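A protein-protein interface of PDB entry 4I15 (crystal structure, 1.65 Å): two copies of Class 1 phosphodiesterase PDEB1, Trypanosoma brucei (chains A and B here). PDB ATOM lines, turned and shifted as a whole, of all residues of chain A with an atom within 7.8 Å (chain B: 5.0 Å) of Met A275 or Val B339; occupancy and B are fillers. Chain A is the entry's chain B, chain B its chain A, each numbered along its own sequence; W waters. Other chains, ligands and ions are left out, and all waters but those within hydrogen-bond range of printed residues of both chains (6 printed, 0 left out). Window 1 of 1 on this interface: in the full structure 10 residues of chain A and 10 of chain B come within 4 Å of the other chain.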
ATOM      1  N   MET A 139     -34.948  11.359 -20.849  1.00  0.00           N
ATOM      2  CA  MET A 139     -33.510  11.113 -20.715  1.00  0.00           C
ATOM      3  C   MET A 139     -32.651  12.200 -21.346  1.00  0.00           C
ATOM      4  O   MET A 139     -31.420  12.086 -21.364  1.00  0.00           O
ATOM      5  CB  MET A 139     -33.133   9.779 -21.369  1.00  0.00           C
ATOM      6  CG  MET A 139     -33.922   8.577 -20.894  1.00  0.00           C
ATOM      7  SD  MET A 139     -33.378   7.088 -21.772  1.00  0.00           S
ATOM      8  CE  MET A 139     -31.598   7.140 -21.404  1.00  0.00           C
ATOM      9  N   GLY A 140     -33.291  13.239 -21.875  1.00  0.00           N
ATOM     10  CA  GLY A 140     -32.549  14.309 -22.524  1.00  0.00           C
ATOM     11  C   GLY A 140     -32.300  14.011 -23.992  1.00  0.00           C
ATOM     12  O   GLY A 140     -31.447  14.635 -24.631  1.00  0.00           O
ATOM     13  N   LEU A 141     -33.048  13.051 -24.529  1.00  0.00           N
ATOM     14  CA  LEU A 141     -32.921  12.659 -25.932  1.00  0.00           C
ATOM     15  C   LEU A 141     -34.309  12.761 -26.564  1.00  0.00           C
ATOM     16  O   LEU A 141     -35.292  12.348 -25.957  1.00  0.00           O
ATOM     17  CB  LEU A 141     -32.414  11.219 -26.030  1.00  0.00           C
ATOM     18  CG  LEU A 141     -31.060  10.909 -25.388  1.00  0.00           C
ATOM     19  CD1 LEU A 141     -30.849   9.401 -25.376  1.00  0.00           C
ATOM     20  CD2 LEU A 141     -29.935  11.612 -26.152  1.00  0.00           C
ATOM     21  N   PHE A 145     -33.833  10.695 -31.850  1.00  0.00           N
ATOM     22  CA  PHE A 145     -32.672   9.932 -31.416  1.00  0.00           C
ATOM     23  C   PHE A 145     -32.982   8.443 -31.347  1.00  0.00           C
ATOM     24  O   PHE A 145     -32.237   7.624 -31.882  1.00  0.00           O
ATOM     25  CB  PHE A 145     -32.176  10.407 -30.049  1.00  0.00           C
ATOM     26  CG  PHE A 145     -31.012   9.608 -29.523  1.00  0.00           C
ATOM     27  CD1 PHE A 145     -31.220   8.452 -28.774  1.00  0.00           C
ATOM     28  CD2 PHE A 145     -29.708   9.980 -29.830  1.00  0.00           C
ATOM     29  CE1 PHE A 145     -30.144   7.672 -28.343  1.00  0.00           C
ATOM     30  CE2 PHE A 145     -28.621   9.210 -29.406  1.00  0.00           C
ATOM     31  CZ  PHE A 145     -28.841   8.052 -28.661  1.00  0.00           C
ATOM     32  N   TYR A 146     -34.087   8.093 -30.696  1.00  0.00           N
ATOM     33  CA  TYR A 146     -34.450   6.688 -30.556  1.00  0.00           C
ATOM     34  C   TYR A 146     -34.700   6.004 -31.890  1.00  0.00           C
ATOM     35  O   TYR A 146     -34.365   4.832 -32.067  1.00  0.00           O
ATOM     36  CB  TYR A 146     -35.687   6.543 -29.665  1.00  0.00           C
ATOM     37  CG  TYR A 146     -35.459   7.014 -28.249  1.00  0.00           C
ATOM     38  CD1 TYR A 146     -35.629   8.355 -27.902  1.00  0.00           C
ATOM     39  CD2 TYR A 146     -35.031   6.127 -27.263  1.00  0.00           C
ATOM     40  CE1 TYR A 146     -35.377   8.800 -26.606  1.00  0.00           C
ATOM     41  CE2 TYR A 146     -34.774   6.559 -25.965  1.00  0.00           C
ATOM     42  CZ  TYR A 146     -34.948   7.897 -25.646  1.00  0.00           C
ATOM     43  OH  TYR A 146     -34.687   8.327 -24.368  1.00  0.00           O
ATOM     44  N   THR A 149     -31.166   5.854 -34.092  1.00  0.00           N
ATOM     45  CA  THR A 149     -30.210   4.878 -33.579  1.00  0.00           C
ATOM     46  C   THR A 149     -30.810   3.485 -33.439  1.00  0.00           C
ATOM     47  O   THR A 149     -30.115   2.534 -33.081  1.00  0.00           O
ATOM     48  CB  THR A 149     -29.684   5.299 -32.194  1.00  0.00           C
ATOM     49  OG1 THR A 149     -30.780   5.387 -31.278  1.00  0.00           O
ATOM     50  CG2 THR A 149     -28.993   6.651 -32.267  1.00  0.00           C
ATOM     51  N   SER A 151     -32.822   2.455 -31.222  1.00  0.00           N
ATOM     52  CA  SER A 151     -32.751   2.126 -29.806  1.00  0.00           C
ATOM     53  C   SER A 151     -33.983   1.256 -29.528  1.00  0.00           C
ATOM     54  O   SER A 151     -34.998   1.398 -30.200  1.00  0.00           O
ATOM     55  CB  SER A 151     -32.816   3.418 -28.986  1.00  0.00           C
ATOM     56  OG  SER A 151     -32.584   3.165 -27.616  1.00  0.00           O
ATOM     57  N   GLU A 268     -28.606  20.515 -23.172  1.00  0.00           N
ATOM     58  CA  GLU A 268     -29.180  19.187 -23.305  1.00  0.00           C
ATOM     59  C   GLU A 268     -29.088  18.729 -24.758  1.00  0.00           C
ATOM     60  O   GLU A 268     -28.731  17.585 -25.025  1.00  0.00           O
ATOM     61  CB  GLU A 268     -30.632  19.176 -22.823  1.00  0.00           C
ATOM     62  CG  GLU A 268     -31.239  17.788 -22.792  1.00  0.00           C
ATOM     63  CD  GLU A 268     -32.617  17.771 -22.164  1.00  0.00           C
ATOM     64  OE1 GLU A 268     -32.723  18.010 -20.940  1.00  0.00           O
ATOM     65  OE2 GLU A 268     -33.593  17.514 -22.901  1.00  0.00           O
ATOM     66  N   PHE A 269     -29.396  19.622 -25.695  1.00  0.00           N
ATOM     67  CA  PHE A 269     -29.317  19.293 -27.119  1.00  0.00           C
ATOM     68  C   PHE A 269     -27.886  18.894 -27.483  1.00  0.00           C
ATOM     69  O   PHE A 269     -27.655  17.923 -28.211  1.00  0.00           O
ATOM     70  CB  PHE A 269     -29.723  20.492 -27.988  1.00  0.00           C
ATOM     71  CG  PHE A 269     -31.206  20.774 -28.009  1.00  0.00           C
ATOM     72  CD1 PHE A 269     -32.120  19.871 -27.471  1.00  0.00           C
ATOM     73  CD2 PHE A 269     -31.687  21.939 -28.601  1.00  0.00           C
ATOM     74  CE1 PHE A 269     -33.492  20.124 -27.526  1.00  0.00           C
ATOM     75  CE2 PHE A 269     -33.054  22.200 -28.662  1.00  0.00           C
ATOM     76  CZ  PHE A 269     -33.959  21.290 -28.123  1.00  0.00           C
ATOM     77  N   TYR A 270     -26.926  19.660 -26.978  1.00  0.00           N
ATOM     78  CA  TYR A 270     -25.521  19.386 -27.246  1.00  0.00           C
ATOM     79  C   TYR A 270     -25.117  18.008 -26.728  1.00  0.00           C
ATOM     80  O   TYR A 270     -24.312  17.319 -27.353  1.00  0.00           O
ATOM     81  CB  TYR A 270     -24.651  20.470 -26.603  1.00  0.00           C
ATOM     82  CG  TYR A 270     -24.632  21.788 -27.352  1.00  0.00           C
ATOM     83  CD1 TYR A 270     -24.084  22.927 -26.769  1.00  0.00           C
ATOM     84  CD2 TYR A 270     -25.121  21.890 -28.658  1.00  0.00           C
ATOM     85  CE1 TYR A 270     -24.018  24.130 -27.463  1.00  0.00           C
ATOM     86  CE2 TYR A 270     -25.058  23.091 -29.362  1.00  0.00           C
ATOM     87  CZ  TYR A 270     -24.503  24.206 -28.756  1.00  0.00           C
ATOM     88  OH  TYR A 270     -24.419  25.401 -29.443  1.00  0.00           O
ATOM     89  N   ARG A 271     -25.672  17.603 -25.589  1.00  0.00           N
ATOM     90  CA  ARG A 271     -25.356  16.291 -25.039  1.00  0.00           C
ATOM     91  C   ARG A 271     -25.955  15.189 -25.914  1.00  0.00           C
ATOM     92  O   ARG A 271     -25.410  14.086 -25.995  1.00  0.00           O
ATOM     93  CB  ARG A 271     -25.854  16.167 -23.596  1.00  0.00           C
ATOM     94  CG  ARG A 271     -25.124  17.083 -22.613  1.00  0.00           C
ATOM     95  CD  ARG A 271     -25.511  16.793 -21.167  1.00  0.00           C
ATOM     96  NE  ARG A 271     -24.892  17.742 -20.245  1.00  0.00           N
ATOM     97  CZ  ARG A 271     -25.032  17.710 -18.922  1.00  0.00           C
ATOM     98  NH1 ARG A 271     -25.775  16.774 -18.346  1.00  0.00           N
ATOM     99  NH2 ARG A 271     -24.432  18.625 -18.173  1.00  0.00           N
ATOM    100  N   GLN A 272     -27.077  15.471 -26.572  1.00  0.00           N
ATOM    101  CA  GLN A 272     -27.662  14.467 -27.450  1.00  0.00           C
ATOM    102  C   GLN A 272     -26.742  14.349 -28.656  1.00  0.00           C
ATOM    103  O   GLN A 272     -26.471  13.253 -29.142  1.00  0.00           O
ATOM    104  CB  GLN A 272     -29.064  14.862 -27.928  1.00  0.00           C
ATOM    105  CG  GLN A 272     -29.577  13.903 -29.005  1.00  0.00           C
ATOM    106  CD  GLN A 272     -31.031  14.124 -29.377  1.00  0.00           C
ATOM    107  OE1 GLN A 272     -31.863  14.395 -28.519  1.00  0.00           O
ATOM    108  NE2 GLN A 272     -31.343  13.985 -30.665  1.00  0.00           N
ATOM    109  N   GLY A 273     -26.269  15.495 -29.135  1.00  0.00           N
ATOM    110  CA  GLY A 273     -25.371  15.508 -30.270  1.00  0.00           C
ATOM    111  C   GLY A 273     -24.114  14.713 -29.968  1.00  0.00           C
ATOM    112  O   GLY A 273     -23.613  13.983 -30.826  1.00  0.00           O
ATOM    113  N   ASP A 274     -23.597  14.849 -28.746  1.00  0.00           N
ATOM    114  CA  ASP A 274     -22.393  14.115 -28.364  1.00  0.00           C
ATOM    115  C   ASP A 274     -22.653  12.614 -28.378  1.00  0.00           C
ATOM    116  O   ASP A 274     -21.816  11.841 -28.837  1.00  0.00           O
ATOM    117  CB  ASP A 274     -21.904  14.548 -26.977  1.00  0.00           C
ATOM    118  CG  ASP A 274     -21.357  15.963 -26.969  1.00  0.00           C
ATOM    119  OD1 ASP A 274     -21.032  16.488 -28.057  1.00  0.00           O
ATOM    120  OD2 ASP A 274     -21.235  16.548 -25.872  1.00  0.00           O
ATOM    121  N   MET A 275     -23.815  12.201 -27.882  1.00  0.00           N
ATOM    122  CA  MET A 275     -24.160  10.785 -27.880  1.00  0.00           C
ATOM    123  C   MET A 275     -24.364  10.286 -29.308  1.00  0.00           C
ATOM    124  O   MET A 275     -24.070   9.132 -29.616  1.00  0.00           O
ATOM    125  CB  MET A 275     -25.419  10.536 -27.045  1.00  0.00           C
ATOM    126  CG  MET A 275     -25.127  10.394 -25.551  1.00  0.00           C
ATOM    127  SD  MET A 275     -26.596  10.124 -24.562  1.00  0.00           S
ATOM    128  CE  MET A 275     -27.069   8.490 -25.123  1.00  0.00           C
ATOM    129  N   GLU A 276     -24.870  11.154 -30.179  1.00  0.00           N
ATOM    130  CA  GLU A 276     -25.078  10.769 -31.570  1.00  0.00           C
ATOM    131  C   GLU A 276     -23.724  10.566 -32.254  1.00  0.00           C
ATOM    132  O   GLU A 276     -23.571   9.679 -33.093  1.00  0.00           O
ATOM    133  CB  GLU A 276     -25.912  11.832 -32.296  1.00  0.00           C
ATOM    134  CG  GLU A 276     -27.344  11.926 -31.761  1.00  0.00           C
ATOM    135  CD  GLU A 276     -28.169  13.024 -32.422  1.00  0.00           C
ATOM    136  OE1 GLU A 276     -27.622  14.119 -32.656  1.00  0.00           O
ATOM    137  OE2 GLU A 276     -29.373  12.798 -32.686  1.00  0.00           O
ATOM    138  N   LYS A 277     -22.735  11.379 -31.891  1.00  0.00           N
ATOM    139  CA  LYS A 277     -21.406  11.219 -32.476  1.00  0.00           C
ATOM    140  C   LYS A 277     -20.836   9.869 -32.036  1.00  0.00           C
ATOM    141  O   LYS A 277     -20.174   9.177 -32.812  1.00  0.00           O
ATOM    142  CB  LYS A 277     -20.481  12.360 -32.032  1.00  0.00           C
ATOM    143  CG  LYS A 277     -20.854  13.710 -32.618  1.00  0.00           C
ATOM    144  CD  LYS A 277     -19.899  14.819 -32.191  1.00  0.00           C
ATOM    145  CE  LYS A 277     -20.382  16.174 -32.699  1.00  0.00           C
ATOM    146  NZ  LYS A 277     -19.501  17.296 -32.267  1.00  0.00           N
ATOM    147  N   GLU A 278     -21.109   9.486 -30.792  1.00  0.00           N
ATOM    148  CA  GLU A 278     -20.628   8.213 -30.267  1.00  0.00           C
ATOM    149  C   GLU A 278     -21.313   7.032 -30.963  1.00  0.00           C
ATOM    150  O   GLU A 278     -20.706   5.977 -31.150  1.00  0.00           O
ATOM    151  CB  GLU A 278     -20.864   8.141 -28.754  1.00  0.00           C
ATOM    152  CG  GLU A 278     -20.014   7.089 -28.050  1.00  0.00           C
ATOM    153  CD  GLU A 278     -20.592   5.693 -28.148  1.00  0.00           C
ATOM    154  OE1 GLU A 278     -19.819   4.718 -28.007  1.00  0.00           O
ATOM    155  OE2 GLU A 278     -21.820   5.571 -28.351  1.00  0.00           O
ATOM    156  N   ARG A 279     -22.575   7.213 -31.347  1.00  0.00           N
ATOM    157  CA  ARG A 279     -23.322   6.161 -32.031  1.00  0.00           C
ATOM    158  C   ARG A 279     -23.067   6.201 -33.531  1.00  0.00           C
ATOM    159  O   ARG A 279     -23.511   5.322 -34.265  1.00  0.00           O
ATOM    160  CB  ARG A 279     -24.827   6.302 -31.775  1.00  0.00           C
ATOM    161  CG  ARG A 279     -25.260   6.023 -30.339  1.00  0.00           C
ATOM    162  CD  ARG A 279     -24.747   4.673 -29.862  1.00  0.00           C
ATOM    163  NE  ARG A 279     -25.198   3.572 -30.710  1.00  0.00           N
ATOM    164  CZ  ARG A 279     -26.431   3.074 -30.706  1.00  0.00           C
ATOM    165  NH1 ARG A 279     -27.353   3.575 -29.895  1.00  0.00           N
ATOM    166  NH2 ARG A 279     -26.740   2.065 -31.512  1.00  0.00           N
ATOM    167  N   GLY A 280     -22.358   7.230 -33.983  1.00  0.00           N
ATOM    168  CA  GLY A 280     -22.057   7.354 -35.398  1.00  0.00           C
ATOM    169  C   GLY A 280     -23.235   7.736 -36.281  1.00  0.00           C
ATOM    170  O   GLY A 280     -23.269   7.373 -37.461  1.00  0.00           O
ATOM    171  N   VAL A 281     -24.204   8.459 -35.729  1.00  0.00           N
ATOM    172  CA  VAL A 281     -25.358   8.874 -36.515  1.00  0.00           C
ATOM    173  C   VAL A 281     -25.315  10.365 -36.818  1.00  0.00           C
ATOM    174  O   VAL A 281     -24.465  11.094 -36.300  1.00  0.00           O
ATOM    175  CB  VAL A 281     -26.695   8.541 -35.803  1.00  0.00           C
ATOM    176  CG1 VAL A 281     -26.818   7.030 -35.612  1.00  0.00           C
ATOM    177  CG2 VAL A 281     -26.780   9.268 -34.473  1.00  0.00           C
ATOM    178  N   VAL A 283     -25.803  14.248 -36.888  1.00  0.00           N
ATOM    179  CA  VAL A 283     -25.957  15.267 -35.860  1.00  0.00           C
ATOM    180  C   VAL A 283     -26.407  16.560 -36.534  1.00  0.00           C
ATOM    181  O   VAL A 283     -25.664  17.142 -37.326  1.00  0.00           O
ATOM    182  CB  VAL A 283     -24.632  15.535 -35.109  1.00  0.00           C
ATOM    183  CG1 VAL A 283     -24.839  16.628 -34.066  1.00  0.00           C
ATOM    184  CG2 VAL A 283     -24.142  14.253 -34.443  1.00  0.00           C
ATOM    185  N   PHE A 287     -27.874  20.538 -32.614  1.00  0.00           N
ATOM    186  CA  PHE A 287     -27.336  19.686 -31.558  1.00  0.00           C
ATOM    187  C   PHE A 287     -25.817  19.542 -31.629  1.00  0.00           C
ATOM    188  O   PHE A 287     -25.227  18.812 -30.832  1.00  0.00           O
ATOM    189  CB  PHE A 287     -27.969  18.289 -31.633  1.00  0.00           C
ATOM    190  CG  PHE A 287     -29.475  18.294 -31.585  1.00  0.00           C
ATOM    191  CD1 PHE A 287     -30.220  18.784 -32.656  1.00  0.00           C
ATOM    192  CD2 PHE A 287     -30.149  17.817 -30.464  1.00  0.00           C
ATOM    193  CE1 PHE A 287     -31.618  18.799 -32.609  1.00  0.00           C
ATOM    194  CE2 PHE A 287     -31.547  17.826 -30.408  1.00  0.00           C
ATOM    195  CZ  PHE A 287     -32.282  18.319 -31.484  1.00  0.00           C
ATOM    196  N   PHE B 255     -17.703  15.678 -21.924  1.00  0.00           N
ATOM    197  CA  PHE B 255     -17.869  14.382 -22.573  1.00  0.00           C
ATOM    198  C   PHE B 255     -17.204  14.176 -23.935  1.00  0.00           C
ATOM    199  O   PHE B 255     -16.432  13.236 -24.105  1.00  0.00           O
ATOM    200  CB  PHE B 255     -19.354  14.045 -22.702  1.00  0.00           C
ATOM    201  CG  PHE B 255     -19.611  12.613 -23.071  1.00  0.00           C
ATOM    202  CD1 PHE B 255     -19.561  11.614 -22.102  1.00  0.00           C
ATOM    203  CD2 PHE B 255     -19.895  12.257 -24.386  1.00  0.00           C
ATOM    204  CE1 PHE B 255     -19.793  10.283 -22.436  1.00  0.00           C
ATOM    205  CE2 PHE B 255     -20.127  10.928 -24.732  1.00  0.00           C
ATOM    206  CZ  PHE B 255     -20.078   9.939 -23.754  1.00  0.00           C
ATOM    207  N   ALA B 296     -18.026   2.417 -23.799  1.00  0.00           N
ATOM    208  CA  ALA B 296     -18.816   2.797 -22.632  1.00  0.00           C
ATOM    209  C   ALA B 296     -18.433   2.019 -21.377  1.00  0.00           C
ATOM    210  O   ALA B 296     -18.258   2.605 -20.311  1.00  0.00           O
ATOM    211  CB  ALA B 296     -20.312   2.615 -22.921  1.00  0.00           C
ATOM    212  N   GLN B 335     -23.512   9.750 -18.374  1.00  0.00           N
ATOM    213  CA  GLN B 335     -23.673   9.842 -19.820  1.00  0.00           C
ATOM    214  C   GLN B 335     -23.343   8.492 -20.467  1.00  0.00           C
ATOM    215  O   GLN B 335     -24.033   8.060 -21.390  1.00  0.00           O
ATOM    216  CB  GLN B 335     -22.765  10.936 -20.382  1.00  0.00           C
ATOM    217  CG  GLN B 335     -22.972  11.231 -21.860  1.00  0.00           C
ATOM    218  CD  GLN B 335     -23.907  12.400 -22.105  1.00  0.00           C
ATOM    219  OE1 GLN B 335     -23.636  13.528 -21.689  1.00  0.00           O
ATOM    220  NE2 GLN B 335     -25.017  12.137 -22.786  1.00  0.00           N
ATOM    221  N   TRP B 336     -22.284   7.828 -20.001  1.00  0.00           N
ATOM    222  CA  TRP B 336     -21.948   6.518 -20.560  1.00  0.00           C
ATOM    223  C   TRP B 336     -23.040   5.517 -20.188  1.00  0.00           C
ATOM    224  O   TRP B 336     -23.332   4.592 -20.951  1.00  0.00           O
ATOM    225  CB  TRP B 336     -20.582   6.023 -20.058  1.00  0.00           C
ATOM    226  CG  TRP B 336     -19.420   6.731 -20.706  1.00  0.00           C
ATOM    227  CD1 TRP B 336     -18.501   7.534 -20.089  1.00  0.00           C
ATOM    228  CD2 TRP B 336     -19.073   6.724 -22.099  1.00  0.00           C
ATOM    229  NE1 TRP B 336     -17.606   8.027 -21.011  1.00  0.00           N
ATOM    230  CE2 TRP B 336     -17.933   7.547 -22.251  1.00  0.00           C
ATOM    231  CE3 TRP B 336     -19.615   6.104 -23.235  1.00  0.00           C
ATOM    232  CZ2 TRP B 336     -17.323   7.765 -23.491  1.00  0.00           C
ATOM    233  CZ3 TRP B 336     -19.008   6.323 -24.470  1.00  0.00           C
ATOM    234  CH2 TRP B 336     -17.872   7.147 -24.586  1.00  0.00           C
ATOM    235  N   GLU B 337     -23.645   5.699 -19.014  1.00  0.00           N
ATOM    236  CA  GLU B 337     -24.720   4.804 -18.583  1.00  0.00           C
ATOM    237  C   GLU B 337     -25.935   4.977 -19.498  1.00  0.00           C
ATOM    238  O   GLU B 337     -26.649   4.011 -19.779  1.00  0.00           O
ATOM    239  CB  GLU B 337     -25.105   5.079 -17.121  1.00  0.00           C
ATOM    240  CG  GLU B 337     -24.113   4.516 -16.096  1.00  0.00           C
ATOM    241  CD  GLU B 337     -24.171   2.993 -15.972  1.00  0.00           C
ATOM    242  OE1 GLU B 337     -24.812   2.340 -16.826  1.00  0.00           O
ATOM    243  OE2 GLU B 337     -23.568   2.444 -15.022  1.00  0.00           O
ATOM    244  N   ARG B 338     -26.166   6.205 -19.962  1.00  0.00           N
ATOM    245  CA  ARG B 338     -27.283   6.479 -20.869  1.00  0.00           C
ATOM    246  C   ARG B 338     -26.983   5.831 -22.218  1.00  0.00           C
ATOM    247  O   ARG B 338     -27.893   5.386 -22.915  1.00  0.00           O
ATOM    248  CB  ARG B 338     -27.487   7.988 -21.044  1.00  0.00           C
ATOM    249  CG  ARG B 338     -27.839   8.711 -19.750  1.00  0.00           C
ATOM    250  CD  ARG B 338     -27.788  10.224 -19.916  1.00  0.00           C
ATOM    251  NE  ARG B 338     -27.809  10.904 -18.622  1.00  0.00           N
ATOM    252  CZ  ARG B 338     -27.669  12.214 -18.462  1.00  0.00           C
ATOM    253  NH1 ARG B 338     -27.495  12.998 -19.520  1.00  0.00           N
ATOM    254  NH2 ARG B 338     -27.705  12.744 -17.244  1.00  0.00           N
ATOM    255  N   VAL B 339     -25.705   5.778 -22.589  1.00  0.00           N
ATOM    256  CA  VAL B 339     -25.327   5.140 -23.846  1.00  0.00           C
ATOM    257  C   VAL B 339     -25.654   3.651 -23.736  1.00  0.00           C
ATOM    258  O   VAL B 339     -26.157   3.044 -24.680  1.00  0.00           O
ATOM    259  CB  VAL B 339     -23.813   5.310 -24.156  1.00  0.00           C
ATOM    260  CG1 VAL B 339     -23.414   4.418 -25.329  1.00  0.00           C
ATOM    261  CG2 VAL B 339     -23.512   6.764 -24.503  1.00  0.00           C
ATOM    262  N   LEU B 340     -25.380   3.060 -22.577  1.00  0.00           N
ATOM    263  CA  LEU B 340     -25.671   1.649 -22.382  1.00  0.00           C
ATOM    264  C   LEU B 340     -27.177   1.419 -22.335  1.00  0.00           C
ATOM    265  O   LEU B 340     -27.689   0.491 -22.955  1.00  0.00           O
ATOM    266  CB  LEU B 340     -25.051   1.138 -21.080  1.00  0.00           C
ATOM    267  CG  LEU B 340     -23.524   1.102 -20.998  1.00  0.00           C
ATOM    268  CD1 LEU B 340     -23.110   0.594 -19.626  1.00  0.00           C
ATOM    269  CD2 LEU B 340     -22.968   0.194 -22.083  1.00  0.00           C
ATOM    270  N   GLU B 341     -27.881   2.278 -21.608  1.00  0.00           N
ATOM    271  CA  GLU B 341     -29.325   2.131 -21.461  1.00  0.00           C
ATOM    272  C   GLU B 341     -30.094   2.200 -22.777  1.00  0.00           C
ATOM    273  O   GLU B 341     -31.133   1.548 -22.929  1.00  0.00           O
ATOM    274  CB  GLU B 341     -29.860   3.190 -20.493  1.00  0.00           C
ATOM    275  CG  GLU B 341     -31.345   3.043 -20.192  1.00  0.00           C
ATOM    276  CD  GLU B 341     -31.862   4.109 -19.250  1.00  0.00           C
ATOM    277  OE1 GLU B 341     -33.058   4.052 -18.896  1.00  0.00           O
ATOM    278  OE2 GLU B 341     -31.080   5.005 -18.866  1.00  0.00           O
ATOM    279  N   THR B 342     -29.589   2.978 -23.727  1.00  0.00           N
ATOM    280  CA  THR B 342     -30.263   3.132 -25.014  1.00  0.00           C
ATOM    281  C   THR B 342     -29.708   2.264 -26.137  1.00  0.00           C
ATOM    282  O   THR B 342     -30.168   2.355 -27.276  1.00  0.00           O
ATOM    283  CB  THR B 342     -30.231   4.601 -25.489  1.00  0.00           C
ATOM    284  OG1 THR B 342     -28.874   5.060 -25.554  1.00  0.00           O
ATOM    285  CG2 THR B 342     -31.016   5.484 -24.530  1.00  0.00           C
ATOM    286  N   ARG B 343     -28.725   1.424 -25.830  1.00  0.00           N
ATOM    287  CA  ARG B 343     -28.143   0.570 -26.860  1.00  0.00           C
ATOM    288  C   ARG B 343     -29.122  -0.522 -27.287  1.00  0.00           C
ATOM    289  O   ARG B 343     -29.192  -0.802 -28.506  1.00  0.00           O
ATOM    290  CB  ARG B 343     -26.843  -0.077 -26.369  1.00  0.00           C
ATOM    291  CG  ARG B 343     -25.870  -0.378 -27.504  1.00  0.00           C
ATOM    292  CD  ARG B 343     -24.685  -1.232 -27.065  1.00  0.00           C
ATOM    293  NE  ARG B 343     -25.043  -2.643 -26.964  1.00  0.00           N
ATOM    294  CZ  ARG B 343     -24.168  -3.635 -26.846  1.00  0.00           C
ATOM    295  NH1 ARG B 343     -22.865  -3.377 -26.808  1.00  0.00           N
ATOM    296  NH2 ARG B 343     -24.592  -4.886 -26.771  1.00  0.00           N
ATOM    297  OXT ARG B 343     -29.793  -1.094 -26.396  1.00  0.00           O
HETATM  298  O   HOH W   1     -18.809  17.456 -24.677  1.00  0.00           O
HETATM  299  O   HOH W   2     -19.613   2.531 -26.382  1.00  0.00           O
HETATM  300  O   HOH W   3     -27.434  12.845 -23.438  1.00  0.00           O
HETATM  301  O   HOH W   4     -22.090  16.048 -23.558  1.00  0.00           O
HETATM  302  O   HOH W   5     -29.385  14.522 -20.861  1.00  0.00           O
HETATM  303  O   HOH W   6     -26.990   4.767 -27.227  1.00  0.00           O
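Of the 11 printed residues of chain B, 7 touch a printed residue of chain A.
Printed residues of chain B that touch a printed residue of chain A: Phe B255, Gln B335, Trp B336, Arg B338, Val B339, Glu B341 and Thr B342.
Hydrophobic or aromatic side chains of chain B within 4 Å of the printed part of chain A: Phe B255, Trp B336 and Val B339.
Among the printed residues, no Asp or Glu carboxylate lies within 4 Å of a Lys or Arg side-chain nitrogen of the other chain.
Among the printed residues, pairs that only touch across the chains: Met A139 with Glu B341, Met A139 with Thr B342, Glu A278 with Val B339, Arg A271 with Gln B335, Glu A278 with Trp B336, Met A275 with Arg B338, Met A275 with Thr B342, Met A275 with Val B339 and Asp A274 with Phe B255.
Water W4 lies within hydrogen-bond range of OD2 of Asp A274 and OE1 of Gln B335.
Water W6 lies within hydrogen-bond range of OG1 of Thr B342 (2.5 Å), NH1 of Arg A279 (2.9 Å) and O of Val B339 (3.2 Å).
Water W3 lies within hydrogen-bond range of the side-chain amide nitrogen of Gln B335 (2.6 Å), the side-chain sulfur of Met A275 (3.1 Å) and the backbone carbonyl oxygen of Arg A271 (3.5 Å).
Water W2 lies within hydrogen-bond range of the side-chain carboxylate (OE1) of Glu A278 (2.7 Å) and the backbone NH (N) of Ala B296 (3.0 Å).
Water W5 bridges NH1 of Arg B338 (2.8 Å) and O of Met A139 (3.2 Å).
Water W1 lies within hydrogen-bond range of OD2 of Asp A274 and N of Phe B255.
O of Thr B342 is in hydrogen-bond range of OG of Ser A151 (2.6 Å).
The side-chain amide nitrogen (NE2) of Gln B335 sits at hydrogen-bond distance from the side-chain sulfur (SD) of Met A275 (3.1 Å).
Of the printed residues of chain B, Met A139 touches Glu B341 and Thr B342.
Of the printed residues of chain B, Ser A151 touches Thr B342.
Gln A272 touches none of the printed residues of chain B.
Met A275 touches just these residues of chain B: Gln B335 (3.1 Å), Arg B338 (3.9 Å), Val B339 (3.95 Å) and Thr B342 (3.9 Å).
Of the printed residues of chain B, Glu A278 touches Trp B336 (3.8 Å) and Val B339 (3.6 Å).
Arg A279 touches none of the printed residues of chain B.
Printed residues of chain A within 4 Å of Phe B255: Asp A274 (3.9998 Å).
Of the printed residues of chain A, Val B339 touches Met A275 and Glu A278.
Printed residues of chain A within 4 Å of Glu B341: Met A139.
The nearest printed residue of chain B that does not touch Met A275 is Phe B255 (5.0 Å).
No position is printed for both chains.
The backbone carbonyl oxygen (O) of Val B339 is in hydrogen-bond range of the side-chain hydroxyl (OG1) of Thr B342 (3.5 Å).
O of Tyr A146 sits at hydrogen-bond distance from N of Ser A151 (3.0 Å).
SD of Met A139 is in hydrogen-bond range of OH of Tyr A146 (3.2 Å).
The backbone carbonyl oxygen of Arg B338 lies within hydrogen-bond range of the side-chain hydroxyl of Thr B342, 2.8 Å away.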
